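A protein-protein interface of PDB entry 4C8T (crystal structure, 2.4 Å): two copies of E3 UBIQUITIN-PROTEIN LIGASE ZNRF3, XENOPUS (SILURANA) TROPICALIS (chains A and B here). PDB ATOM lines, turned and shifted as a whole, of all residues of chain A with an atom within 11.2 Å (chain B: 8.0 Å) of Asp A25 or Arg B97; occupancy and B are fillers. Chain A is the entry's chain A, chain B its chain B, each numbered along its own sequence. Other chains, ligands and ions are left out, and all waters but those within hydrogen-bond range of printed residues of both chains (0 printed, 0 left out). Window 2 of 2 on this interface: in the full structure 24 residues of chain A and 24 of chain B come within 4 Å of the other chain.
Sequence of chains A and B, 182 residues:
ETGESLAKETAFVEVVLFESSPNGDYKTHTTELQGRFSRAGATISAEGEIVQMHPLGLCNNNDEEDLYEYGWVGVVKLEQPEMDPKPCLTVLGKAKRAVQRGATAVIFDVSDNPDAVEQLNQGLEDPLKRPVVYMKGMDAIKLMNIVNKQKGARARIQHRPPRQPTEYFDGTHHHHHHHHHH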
ATOM      1  N   LEU A  17     -19.513  -4.900 -31.072  1.00  0.00           N
ATOM      2  CA  LEU A  17     -20.183  -5.063 -29.778  1.00  0.00           C
ATOM      3  C   LEU A  17     -19.366  -5.941 -28.867  1.00  0.00           C
ATOM      4  O   LEU A  17     -18.650  -6.821 -29.318  1.00  0.00           O
ATOM      5  CB  LEU A  17     -21.553  -5.701 -29.938  1.00  0.00           C
ATOM      6  CG  LEU A  17     -22.528  -4.769 -30.638  1.00  0.00           C
ATOM      7  CD1 LEU A  17     -23.840  -5.473 -30.939  1.00  0.00           C
ATOM      8  CD2 LEU A  17     -22.755  -3.562 -29.757  1.00  0.00           C
ATOM      9  N   PHE A  18     -19.493  -5.695 -27.576  1.00  0.00           N
ATOM     10  CA  PHE A  18     -18.661  -6.336 -26.605  1.00  0.00           C
ATOM     11  C   PHE A  18     -19.229  -6.192 -25.180  1.00  0.00           C
ATOM     12  O   PHE A  18     -19.928  -5.231 -24.830  1.00  0.00           O
ATOM     13  CB  PHE A  18     -17.240  -5.752 -26.682  1.00  0.00           C
ATOM     14  CG  PHE A  18     -17.149  -4.314 -26.255  1.00  0.00           C
ATOM     15  CD1 PHE A  18     -17.012  -3.971 -24.913  1.00  0.00           C
ATOM     16  CD2 PHE A  18     -17.214  -3.296 -27.185  1.00  0.00           C
ATOM     17  CE1 PHE A  18     -16.931  -2.641 -24.513  1.00  0.00           C
ATOM     18  CE2 PHE A  18     -17.131  -1.962 -26.786  1.00  0.00           C
ATOM     19  CZ  PHE A  18     -16.989  -1.637 -25.450  1.00  0.00           C
ATOM     20  N   GLU A  19     -18.891  -7.171 -24.364  1.00  0.00           N
ATOM     21  CA  GLU A  19     -19.259  -7.184 -22.962  1.00  0.00           C
ATOM     22  C   GLU A  19     -18.284  -8.144 -22.360  1.00  0.00           C
ATOM     23  O   GLU A  19     -17.785  -9.013 -23.063  1.00  0.00           O
ATOM     24  CB  GLU A  19     -20.685  -7.683 -22.780  1.00  0.00           C
ATOM     25  CG  GLU A  19     -20.954  -9.034 -23.423  1.00  0.00           C
ATOM     26  CD  GLU A  19     -22.434  -9.306 -23.582  1.00  0.00           C
ATOM     27  OE1 GLU A  19     -23.174  -9.079 -22.602  1.00  0.00           O
ATOM     28  OE2 GLU A  19     -22.853  -9.737 -24.682  1.00  0.00           O
ATOM     29  N   SER A  20     -17.975  -8.000 -21.083  1.00  0.00           N
ATOM     30  CA  SER A  20     -16.981  -8.881 -20.503  1.00  0.00           C
ATOM     31  C   SER A  20     -17.578 -10.279 -20.320  1.00  0.00           C
ATOM     32  O   SER A  20     -18.757 -10.432 -19.990  1.00  0.00           O
ATOM     33  CB  SER A  20     -16.438  -8.319 -19.194  1.00  0.00           C
ATOM     34  OG  SER A  20     -17.483  -8.120 -18.275  1.00  0.00           O
ATOM     35  N   SER A  21     -16.770 -11.292 -20.613  1.00  0.00           N
ATOM     36  CA  SER A  21     -17.092 -12.668 -20.258  1.00  0.00           C
ATOM     37  C   SER A  21     -16.649 -12.841 -18.803  1.00  0.00           C
ATOM     38  O   SER A  21     -15.755 -12.122 -18.343  1.00  0.00           O
ATOM     39  CB  SER A  21     -16.394 -13.652 -21.204  1.00  0.00           C
ATOM     40  OG  SER A  21     -17.063 -13.716 -22.450  1.00  0.00           O
ATOM     41  N   PRO A  22     -17.259 -13.795 -18.070  1.00  0.00           N
ATOM     42  CA  PRO A  22     -17.170 -13.757 -16.606  1.00  0.00           C
ATOM     43  C   PRO A  22     -15.768 -13.942 -16.015  1.00  0.00           C
ATOM     44  O   PRO A  22     -15.624 -13.902 -14.801  1.00  0.00           O
ATOM     45  CB  PRO A  22     -18.090 -14.909 -16.173  1.00  0.00           C
ATOM     46  CG  PRO A  22     -18.046 -15.867 -17.303  1.00  0.00           C
ATOM     47  CD  PRO A  22     -17.904 -15.036 -18.548  1.00  0.00           C
ATOM     48  N   ASN A  23     -14.745 -14.086 -16.857  1.00  0.00           N
ATOM     49  CA  ASN A  23     -13.389 -14.466 -16.416  1.00  0.00           C
ATOM     50  C   ASN A  23     -12.277 -13.447 -16.741  1.00  0.00           C
ATOM     51  O   ASN A  23     -11.100 -13.742 -16.540  1.00  0.00           O
ATOM     52  CB  ASN A  23     -13.017 -15.851 -16.994  1.00  0.00           C
ATOM     53  CG  ASN A  23     -13.245 -15.957 -18.508  1.00  0.00           C
ATOM     54  OD1 ASN A  23     -12.297 -15.967 -19.292  1.00  0.00           O
ATOM     55  ND2 ASN A  23     -14.508 -16.064 -18.914  1.00  0.00           N
ATOM     56  N   GLY A  24     -12.651 -12.257 -17.222  1.00  0.00           N
ATOM     57  CA  GLY A  24     -11.685 -11.229 -17.637  1.00  0.00           C
ATOM     58  C   GLY A  24     -11.678 -10.989 -19.143  1.00  0.00           C
ATOM     59  O   GLY A  24     -11.296  -9.910 -19.609  1.00  0.00           O
ATOM     60  N   ASP A  25     -12.106 -12.000 -19.904  1.00  0.00           N
ATOM     61  CA  ASP A  25     -12.072 -11.952 -21.358  1.00  0.00           C
ATOM     62  C   ASP A  25     -13.243 -11.136 -21.883  1.00  0.00           C
ATOM     63  O   ASP A  25     -14.166 -10.809 -21.142  1.00  0.00           O
ATOM     64  CB  ASP A  25     -12.136 -13.364 -21.943  1.00  0.00           C
ATOM     65  CG  ASP A  25     -10.972 -14.239 -21.508  1.00  0.00           C
ATOM     66  OD1 ASP A  25     -10.080 -13.726 -20.797  1.00  0.00           O
ATOM     67  OD2 ASP A  25     -10.937 -15.443 -21.872  1.00  0.00           O
ATOM     68  N   TYR A  26     -13.202 -10.806 -23.169  1.00  0.00           N
ATOM     69  CA  TYR A  26     -14.313 -10.126 -23.801  1.00  0.00           C
ATOM     70  C   TYR A  26     -14.994 -11.040 -24.821  1.00  0.00           C
ATOM     71  O   TYR A  26     -14.317 -11.707 -25.598  1.00  0.00           O
ATOM     72  CB  TYR A  26     -13.839  -8.830 -24.468  1.00  0.00           C
ATOM     73  CG  TYR A  26     -13.703  -7.653 -23.532  1.00  0.00           C
ATOM     74  CD1 TYR A  26     -14.805  -6.895 -23.154  1.00  0.00           C
ATOM     75  CD2 TYR A  26     -12.475  -7.304 -23.043  1.00  0.00           C
ATOM     76  CE1 TYR A  26     -14.670  -5.805 -22.297  1.00  0.00           C
ATOM     77  CE2 TYR A  26     -12.316  -6.244 -22.196  1.00  0.00           C
ATOM     78  CZ  TYR A  26     -13.420  -5.500 -21.810  1.00  0.00           C
ATOM     79  OH  TYR A  26     -13.193  -4.457 -20.959  1.00  0.00           O
ATOM     80  N   LYS A  27     -16.330 -11.091 -24.776  1.00  0.00           N
ATOM     81  CA  LYS A  27     -17.150 -11.651 -25.858  1.00  0.00           C
ATOM     82  C   LYS A  27     -17.503 -10.499 -26.793  1.00  0.00           C
ATOM     83  O   LYS A  27     -17.875  -9.397 -26.362  1.00  0.00           O
ATOM     84  CB  LYS A  27     -18.428 -12.328 -25.340  1.00  0.00           C
ATOM     85  N   THR A  28     -17.382 -10.767 -28.082  1.00  0.00           N
ATOM     86  CA  THR A  28     -17.526  -9.742 -29.079  1.00  0.00           C
ATOM     87  C   THR A  28     -18.365 -10.239 -30.243  1.00  0.00           C
ATOM     88  O   THR A  28     -18.469 -11.446 -30.522  1.00  0.00           O
ATOM     89  CB  THR A  28     -16.166  -9.320 -29.648  1.00  0.00           C
ATOM     90  OG1 THR A  28     -15.560 -10.444 -30.294  1.00  0.00           O
ATOM     91  CG2 THR A  28     -15.239  -8.817 -28.557  1.00  0.00           C
ATOM     92  N   HIS A  29     -18.945  -9.266 -30.930  1.00  0.00           N
ATOM     93  CA  HIS A  29     -19.668  -9.516 -32.130  1.00  0.00           C
ATOM     94  C   HIS A  29     -19.363  -8.377 -33.112  1.00  0.00           C
ATOM     95  O   HIS A  29     -19.567  -7.184 -32.803  1.00  0.00           O
ATOM     96  CB  HIS A  29     -21.129  -9.563 -31.797  1.00  0.00           C
ATOM     97  CG  HIS A  29     -21.994  -9.739 -32.984  1.00  0.00           C
ATOM     98  ND1 HIS A  29     -22.652 -10.915 -33.246  1.00  0.00           N
ATOM     99  CD2 HIS A  29     -22.307  -8.896 -33.988  1.00  0.00           C
ATOM    100  CE1 HIS A  29     -23.349 -10.789 -34.360  1.00  0.00           C
ATOM    101  NE2 HIS A  29     -23.158  -9.571 -34.827  1.00  0.00           N
ATOM    102  N   GLY B  57       2.479  -9.554 -16.341  1.00  0.00           N
ATOM    103  CA  GLY B  57       1.093  -9.182 -16.122  1.00  0.00           C
ATOM    104  C   GLY B  57       0.145  -9.944 -17.013  1.00  0.00           C
ATOM    105  O   GLY B  57      -1.067  -9.785 -16.906  1.00  0.00           O
ATOM    106  N   LEU B  58       0.691 -10.771 -17.904  1.00  0.00           N
ATOM    107  CA  LEU B  58      -0.124 -11.554 -18.839  1.00  0.00           C
ATOM    108  C   LEU B  58      -0.064 -13.080 -18.549  1.00  0.00           C
ATOM    109  O   LEU B  58      -0.047 -13.895 -19.486  1.00  0.00           O
ATOM    110  CB  LEU B  58       0.292 -11.215 -20.283  1.00  0.00           C
ATOM    111  CG  LEU B  58      -0.126  -9.816 -20.791  1.00  0.00           C
ATOM    112  CD1 LEU B  58       0.836  -9.218 -21.816  1.00  0.00           C
ATOM    113  CD2 LEU B  58      -1.533  -9.833 -21.379  1.00  0.00           C
ATOM    114  N   CYS B  59      -0.062 -13.444 -17.251  1.00  0.00           N
ATOM    115  CA  CYS B  59      -0.169 -14.847 -16.806  1.00  0.00           C
ATOM    116  C   CYS B  59      -1.306 -15.116 -15.779  1.00  0.00           C
ATOM    117  O   CYS B  59      -2.273 -14.356 -15.625  1.00  0.00           O
ATOM    118  CB  CYS B  59       1.150 -15.333 -16.196  1.00  0.00           C
ATOM    119  SG  CYS B  59       2.709 -14.641 -16.829  1.00  0.00           S
ATOM    120  N   LEU B  67     -10.292  -5.685 -15.256  1.00  0.00           N
ATOM    121  CA  LEU B  67     -10.828  -5.448 -16.584  1.00  0.00           C
ATOM    122  C   LEU B  67     -10.450  -4.060 -17.086  1.00  0.00           C
ATOM    123  O   LEU B  67     -10.706  -3.066 -16.398  1.00  0.00           O
ATOM    124  CB  LEU B  67     -12.351  -5.595 -16.602  1.00  0.00           C
ATOM    125  N   TYR B  68      -9.849  -4.015 -18.285  1.00  0.00           N
ATOM    126  CA  TYR B  68      -9.575  -2.779 -19.026  1.00  0.00           C
ATOM    127  C   TYR B  68     -10.646  -2.640 -20.128  1.00  0.00           C
ATOM    128  O   TYR B  68     -11.117  -3.649 -20.678  1.00  0.00           O
ATOM    129  CB  TYR B  68      -8.179  -2.837 -19.670  1.00  0.00           C
ATOM    130  CG  TYR B  68      -6.980  -2.767 -18.716  1.00  0.00           C
ATOM    131  CD1 TYR B  68      -6.541  -1.547 -18.186  1.00  0.00           C
ATOM    132  CD2 TYR B  68      -6.259  -3.916 -18.397  1.00  0.00           C
ATOM    133  CE1 TYR B  68      -5.444  -1.486 -17.339  1.00  0.00           C
ATOM    134  CE2 TYR B  68      -5.165  -3.872 -17.550  1.00  0.00           C
ATOM    135  CZ  TYR B  68      -4.757  -2.667 -17.017  1.00  0.00           C
ATOM    136  OH  TYR B  68      -3.648  -2.661 -16.173  1.00  0.00           O
ATOM    137  N   TYR B  70     -12.501  -2.385 -23.509  1.00  0.00           N
ATOM    138  CA  TYR B  70     -12.194  -2.914 -24.847  1.00  0.00           C
ATOM    139  C   TYR B  70     -11.497  -1.929 -25.805  1.00  0.00           C
ATOM    140  O   TYR B  70     -11.884  -0.756 -25.939  1.00  0.00           O
ATOM    141  CB  TYR B  70     -13.472  -3.427 -25.509  1.00  0.00           C
ATOM    142  CG  TYR B  70     -13.216  -4.198 -26.783  1.00  0.00           C
ATOM    143  CD1 TYR B  70     -12.874  -5.548 -26.753  1.00  0.00           C
ATOM    144  CD2 TYR B  70     -13.329  -3.582 -28.018  1.00  0.00           C
ATOM    145  CE1 TYR B  70     -12.651  -6.255 -27.921  1.00  0.00           C
ATOM    146  CE2 TYR B  70     -13.104  -4.283 -29.195  1.00  0.00           C
ATOM    147  CZ  TYR B  70     -12.761  -5.617 -29.153  1.00  0.00           C
ATOM    148  OH  TYR B  70     -12.539  -6.295 -30.353  1.00  0.00           O
ATOM    149  N   TRP B  72      -7.939  -1.388 -26.040  1.00  0.00           N
ATOM    150  CA  TRP B  72      -6.669  -0.775 -25.611  1.00  0.00           C
ATOM    151  C   TRP B  72      -5.443  -1.291 -26.442  1.00  0.00           C
ATOM    152  O   TRP B  72      -5.418  -2.427 -26.958  1.00  0.00           O
ATOM    153  CB  TRP B  72      -6.380  -1.069 -24.132  1.00  0.00           C
ATOM    154  CG  TRP B  72      -6.570  -2.527 -23.703  1.00  0.00           C
ATOM    155  CD1 TRP B  72      -7.752  -3.158 -23.511  1.00  0.00           C
ATOM    156  CD2 TRP B  72      -5.552  -3.498 -23.391  1.00  0.00           C
ATOM    157  NE1 TRP B  72      -7.554  -4.483 -23.117  1.00  0.00           N
ATOM    158  CE2 TRP B  72      -6.203  -4.704 -23.037  1.00  0.00           C
ATOM    159  CE3 TRP B  72      -4.157  -3.476 -23.407  1.00  0.00           C
ATOM    160  CZ2 TRP B  72      -5.505  -5.867 -22.666  1.00  0.00           C
ATOM    161  CZ3 TRP B  72      -3.455  -4.636 -23.020  1.00  0.00           C
ATOM    162  CH2 TRP B  72      -4.139  -5.807 -22.633  1.00  0.00           C
ATOM    163  N   CYS B  88       5.653 -17.961 -18.204  1.00  0.00           N
ATOM    164  CA  CYS B  88       4.279 -18.487 -18.228  1.00  0.00           C
ATOM    165  C   CYS B  88       3.705 -18.697 -19.629  1.00  0.00           C
ATOM    166  O   CYS B  88       2.938 -19.631 -19.846  1.00  0.00           O
ATOM    167  CB  CYS B  88       3.359 -17.532 -17.483  1.00  0.00           C
ATOM    168  SG  CYS B  88       3.258 -15.924 -18.304  1.00  0.00           S
ATOM    169  N   LEU B  89       4.051 -17.816 -20.563  1.00  0.00           N
ATOM    170  CA  LEU B  89       3.665 -17.992 -21.971  1.00  0.00           C
ATOM    171  C   LEU B  89       4.760 -17.570 -22.939  1.00  0.00           C
ATOM    172  O   LEU B  89       5.668 -16.827 -22.579  1.00  0.00           O
ATOM    173  CB  LEU B  89       2.451 -17.123 -22.285  1.00  0.00           C
ATOM    174  CG  LEU B  89       1.097 -17.502 -21.723  1.00  0.00           C
ATOM    175  CD1 LEU B  89       0.108 -16.405 -22.074  1.00  0.00           C
ATOM    176  CD2 LEU B  89       0.651 -18.825 -22.310  1.00  0.00           C
ATOM    177  N   THR B  90       4.630 -17.994 -24.189  1.00  0.00           N
ATOM    178  CA  THR B  90       5.422 -17.402 -25.256  1.00  0.00           C
ATOM    179  C   THR B  90       4.985 -15.951 -25.540  1.00  0.00           C
ATOM    180  O   THR B  90       3.878 -15.511 -25.203  1.00  0.00           O
ATOM    181  CB  THR B  90       5.320 -18.202 -26.570  1.00  0.00           C
ATOM    182  OG1 THR B  90       3.949 -18.253 -27.016  1.00  0.00           O
ATOM    183  CG2 THR B  90       5.872 -19.621 -26.368  1.00  0.00           C
ATOM    184  N   VAL B  91       5.864 -15.212 -26.195  1.00  0.00           N
ATOM    185  CA  VAL B  91       5.610 -13.804 -26.444  1.00  0.00           C
ATOM    186  C   VAL B  91       4.369 -13.682 -27.341  1.00  0.00           C
ATOM    187  O   VAL B  91       3.565 -12.779 -27.192  1.00  0.00           O
ATOM    188  CB  VAL B  91       6.894 -13.104 -26.977  1.00  0.00           C
ATOM    189  CG1 VAL B  91       7.354 -13.704 -28.302  1.00  0.00           C
ATOM    190  CG2 VAL B  91       6.706 -11.604 -27.094  1.00  0.00           C
ATOM    191  N   LEU B  92       4.189 -14.633 -28.236  1.00  0.00           N
ATOM    192  CA  LEU B  92       2.979 -14.708 -29.041  1.00  0.00           C
ATOM    193  C   LEU B  92       1.798 -15.062 -28.131  1.00  0.00           C
ATOM    194  O   LEU B  92       0.733 -14.487 -28.247  1.00  0.00           O
ATOM    195  CB  LEU B  92       3.147 -15.777 -30.127  1.00  0.00           C
ATOM    196  CG  LEU B  92       2.412 -15.692 -31.460  1.00  0.00           C
ATOM    197  CD1 LEU B  92       2.896 -16.843 -32.338  1.00  0.00           C
ATOM    198  CD2 LEU B  92       0.893 -15.706 -31.343  1.00  0.00           C
ATOM    199  N   GLY B  93       1.991 -16.012 -27.229  1.00  0.00           N
ATOM    200  CA  GLY B  93       0.966 -16.349 -26.222  1.00  0.00           C
ATOM    201  C   GLY B  93       0.513 -15.147 -25.392  1.00  0.00           C
ATOM    202  O   GLY B  93      -0.675 -14.942 -25.198  1.00  0.00           O
ATOM    203  N   LYS B  94       1.465 -14.339 -24.952  1.00  0.00           N
ATOM    204  CA  LYS B  94       1.191 -13.150 -24.174  1.00  0.00           C
ATOM    205  C   LYS B  94       0.360 -12.140 -24.936  1.00  0.00           C
ATOM    206  O   LYS B  94      -0.550 -11.516 -24.361  1.00  0.00           O
ATOM    207  CB  LYS B  94       2.478 -12.508 -23.713  1.00  0.00           C
ATOM    208  CG  LYS B  94       3.166 -13.275 -22.592  1.00  0.00           C
ATOM    209  CD  LYS B  94       4.442 -12.563 -22.167  1.00  0.00           C
ATOM    210  CE  LYS B  94       5.360 -13.468 -21.375  1.00  0.00           C
ATOM    211  NZ  LYS B  94       4.886 -13.590 -19.978  1.00  0.00           N
ATOM    212  N   ALA B  95       0.655 -11.996 -26.225  1.00  0.00           N
ATOM    213  CA  ALA B  95      -0.107 -11.102 -27.098  1.00  0.00           C
ATOM    214  C   ALA B  95      -1.569 -11.536 -27.256  1.00  0.00           C
ATOM    215  O   ALA B  95      -2.482 -10.715 -27.266  1.00  0.00           O
ATOM    216  CB  ALA B  95       0.574 -11.032 -28.448  1.00  0.00           C
ATOM    217  N   LYS B  96      -1.746 -12.845 -27.386  1.00  0.00           N
ATOM    218  CA  LYS B  96      -3.026 -13.517 -27.567  1.00  0.00           C
ATOM    219  C   LYS B  96      -3.907 -13.247 -26.351  1.00  0.00           C
ATOM    220  O   LYS B  96      -5.058 -12.951 -26.449  1.00  0.00           O
ATOM    221  CB  LYS B  96      -2.742 -15.028 -27.664  1.00  0.00           C
ATOM    222  CG  LYS B  96      -3.354 -15.756 -28.849  1.00  0.00           C
ATOM    223  CD  LYS B  96      -2.430 -16.829 -29.437  1.00  0.00           C
ATOM    224  CE  LYS B  96      -2.761 -17.177 -30.900  1.00  0.00           C
ATOM    225  NZ  LYS B  96      -4.193 -17.540 -31.183  1.00  0.00           N
ATOM    226  N   ARG B  97      -3.318 -13.359 -25.187  1.00  0.00           N
ATOM    227  CA  ARG B  97      -4.004 -13.195 -23.924  1.00  0.00           C
ATOM    228  C   ARG B  97      -4.464 -11.700 -23.788  1.00  0.00           C
ATOM    229  O   ARG B  97      -5.606 -11.379 -23.427  1.00  0.00           O
ATOM    230  CB  ARG B  97      -2.998 -13.664 -22.851  1.00  0.00           C
ATOM    231  CG  ARG B  97      -3.536 -13.990 -21.490  1.00  0.00           C
ATOM    232  CD  ARG B  97      -4.796 -14.828 -21.456  1.00  0.00           C
ATOM    233  NE  ARG B  97      -5.673 -14.288 -20.416  1.00  0.00           N
ATOM    234  CZ  ARG B  97      -6.994 -14.390 -20.400  1.00  0.00           C
ATOM    235  NH1 ARG B  97      -7.632 -15.035 -21.355  1.00  0.00           N
ATOM    236  NH2 ARG B  97      -7.690 -13.844 -19.409  1.00  0.00           N
ATOM    237  N   ALA B  98      -3.570 -10.797 -24.167  1.00  0.00           N
ATOM    238  CA  ALA B  98      -3.870  -9.386 -24.279  1.00  0.00           C
ATOM    239  C   ALA B  98      -5.117  -9.136 -25.121  1.00  0.00           C
ATOM    240  O   ALA B  98      -6.049  -8.417 -24.733  1.00  0.00           O
ATOM    241  CB  ALA B  98      -2.667  -8.659 -24.885  1.00  0.00           C
ATOM    242  N   VAL B  99      -5.135  -9.731 -26.295  1.00  0.00           N
ATOM    243  CA  VAL B  99      -6.259  -9.522 -27.158  1.00  0.00           C
ATOM    244  C   VAL B  99      -7.520 -10.054 -26.463  1.00  0.00           C
ATOM    245  O   VAL B  99      -8.517  -9.366 -26.374  1.00  0.00           O
ATOM    246  CB  VAL B  99      -6.035 -10.208 -28.523  1.00  0.00           C
ATOM    247  CG1 VAL B  99      -7.341 -10.271 -29.316  1.00  0.00           C
ATOM    248  CG2 VAL B  99      -4.920  -9.503 -29.284  1.00  0.00           C
ATOM    249  N   GLN B 100      -7.484 -11.288 -26.003  1.00  0.00           N
ATOM    250  CA  GLN B 100      -8.637 -11.899 -25.319  1.00  0.00           C
ATOM    251  C   GLN B 100      -9.194 -11.013 -24.196  1.00  0.00           C
ATOM    252  O   GLN B 100     -10.383 -10.992 -23.924  1.00  0.00           O
ATOM    253  CB  GLN B 100      -8.208 -13.229 -24.705  1.00  0.00           C
ATOM    254  CG  GLN B 100      -8.109 -14.374 -25.698  1.00  0.00           C
ATOM    255  CD  GLN B 100      -7.513 -15.608 -25.077  1.00  0.00           C
ATOM    256  OE1 GLN B 100      -7.056 -15.581 -23.925  1.00  0.00           O
ATOM    257  NE2 GLN B 100      -7.501 -16.707 -25.836  1.00  0.00           N
ATOM    258  N   ARG B 101      -8.296 -10.283 -23.572  1.00  0.00           N
ATOM    259  CA  ARG B 101      -8.626  -9.289 -22.602  1.00  0.00           C
ATOM    260  C   ARG B 101      -8.883  -7.932 -23.245  1.00  0.00           C
ATOM    261  O   ARG B 101      -8.618  -6.886 -22.625  1.00  0.00           O
ATOM    262  CB  ARG B 101      -7.463  -9.204 -21.611  1.00  0.00           C
ATOM    263  CG  ARG B 101      -7.178 -10.536 -20.919  1.00  0.00           C
ATOM    264  CD  ARG B 101      -5.875 -10.584 -20.131  1.00  0.00           C
ATOM    265  NE  ARG B 101      -5.728  -9.422 -19.249  1.00  0.00           N
ATOM    266  CZ  ARG B 101      -4.763  -9.243 -18.349  1.00  0.00           C
ATOM    267  NH1 ARG B 101      -3.840 -10.168 -18.134  1.00  0.00           N
ATOM    268  NH2 ARG B 101      -4.725  -8.107 -17.649  1.00  0.00           N
ATOM    269  N   GLY B 102      -9.371  -7.929 -24.488  1.00  0.00           N
ATOM    270  CA  GLY B 102      -9.785  -6.680 -25.174  1.00  0.00           C
ATOM    271  C   GLY B 102      -8.710  -5.755 -25.748  1.00  0.00           C
ATOM    272  O   GLY B 102      -8.992  -4.589 -26.042  1.00  0.00           O
ATOM    273  N   ALA B 103      -7.469  -6.202 -25.894  1.00  0.00           N
ATOM    274  CA  ALA B 103      -6.487  -5.349 -26.593  1.00  0.00           C
ATOM    275  C   ALA B 103      -6.751  -5.340 -28.138  1.00  0.00           C
ATOM    276  O   ALA B 103      -6.957  -6.382 -28.754  1.00  0.00           O
ATOM    277  CB  ALA B 103      -5.066  -5.792 -26.279  1.00  0.00           C
ATOM    278  N   VAL B 106      -1.019  -4.938 -29.800  1.00  0.00           N
ATOM    279  CA  VAL B 106       0.039  -5.080 -28.822  1.00  0.00           C
ATOM    280  C   VAL B 106       1.305  -4.546 -29.434  1.00  0.00           C
ATOM    281  O   VAL B 106       1.627  -4.889 -30.573  1.00  0.00           O
ATOM    282  CB  VAL B 106       0.287  -6.550 -28.465  1.00  0.00           C
ATOM    283  CG1 VAL B 106       1.292  -6.663 -27.341  1.00  0.00           C
ATOM    284  CG2 VAL B 106      -1.013  -7.221 -28.069  1.00  0.00           C
ATOM    285  N   LEU B 128      -2.718 -13.609 -35.396  1.00  0.00           N
ATOM    286  CA  LEU B 128      -3.804 -12.889 -34.773  1.00  0.00           C
ATOM    287  C   LEU B 128      -4.398 -11.967 -35.794  1.00  0.00           C
ATOM    288  O   LEU B 128      -3.709 -11.526 -36.734  1.00  0.00           O
ATOM    289  CB  LEU B 128      -3.261 -12.057 -33.630  1.00  0.00           C
ATOM    290  CG  LEU B 128      -2.696 -12.886 -32.481  1.00  0.00           C
ATOM    291  CD1 LEU B 128      -2.081 -11.995 -31.420  1.00  0.00           C
ATOM    292  CD2 LEU B 128      -3.811 -13.746 -31.913  1.00  0.00           C
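Phe A18 touches Tyr B70 (CD1 to CB, 3.6 Å).
Asp A25 touches Gln B100.
CD2 of Tyr A26 touches C of Arg B101 (3.7 Å).
Gly B102 touches Tyr A26.
Thr A28 touches Tyr B70 (CG2 to CE1, 3.7 Å).
The guanidinium group (NH2) of Arg B97 lies within salt-bridge range of the side-chain carboxylate (OD1) of Asp A25 (2.8 Å).
OH of Tyr A26 lies within hydrogen-bond range of N of Tyr B70, at 3.4 Å.
The backbone carbonyl oxygen (O) of Gln B100 is in hydrogen-bond range of the backbone NH (N) of Tyr A26 (2.9 Å).
The side-chain hydroxyl (OH) of Tyr A26 sits close to the backbone carbonyl oxygen (O) of Tyr B68, 2.2 Å away.
OD2 of Asp A25 sits close to OD1 of Asn A23 (3.0 Å).
The guanidinium group of Arg B101 lies within hydrogen-bond range of the backbone carbonyl oxygen of Gly B57.
NE1 of Trp B72 lies within hydrogen-bond range of O of Arg B101, at 2.7 Å.
NE1 of Trp B72 lies close to O of Gly B102 (3.3 Å).
NH1 of Arg B97 is in hydrogen-bond range of OE1 of Gln B100.
SG of Cys B88 is disulfide-bonded to SG of Cys B59 (2.0 Å).
No position is printed for both chains.
Of the 25 printed residues of chain B, 6 touch a printed residue of chain A.
Hydrophobic or aromatic side chains of chain B within 4 Å of the printed part of chain A: Tyr B70.
Among the printed residues, 9 pairs touch across the chains.
Among the printed residues, Asp or Glu carboxylates within 4 Å of a Lys or Arg side-chain nitrogen of the other chain: Asp A25 with Arg B97 (2.8 Å).
Of chain B, only Arg B97 (2.8 Å) and Gln B100 (3.2 Å) come within 4 Å of Asp A25.
Arg B97 touches just one residue of chain A: Asp A25.
No residue of chain A comes within 4 Å of Gly B93.
No residue of chain A comes within 4 Å of Ala B98.
No residue of chain A comes within 4 Å of Val B99.
Of chain A, only Asp A25 and Tyr A26 come within 4 Å of Gln B100.
Arg B101 touches one residue of chain A.
Of the printed residues of chain B, Tyr A26 touches Tyr B68 (2.2 Å), Tyr B70 (3.4 Å), Gln B100 (2.9 Å), Arg B101 (3.7 Å) and Gly B102 (3.5 Å).
Of the printed residues of chain B, Thr A28 touches Tyr B70.
Printed residues of chain A within 4 Å of Tyr B68: Tyr A26 (2.2 Å).
Printed residues of chain A within 4 Å of Tyr B70: Phe A18 (3.6 Å), Tyr A26 (3.4 Å) and Thr A28 (3.7 Å).
The nearest residue of chain B that does not touch Asp A25 is Arg B101 (4.3 Å).
The nearest printed residue of chain A that does not touch Tyr B70 is Leu A17 (6.0 Å).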
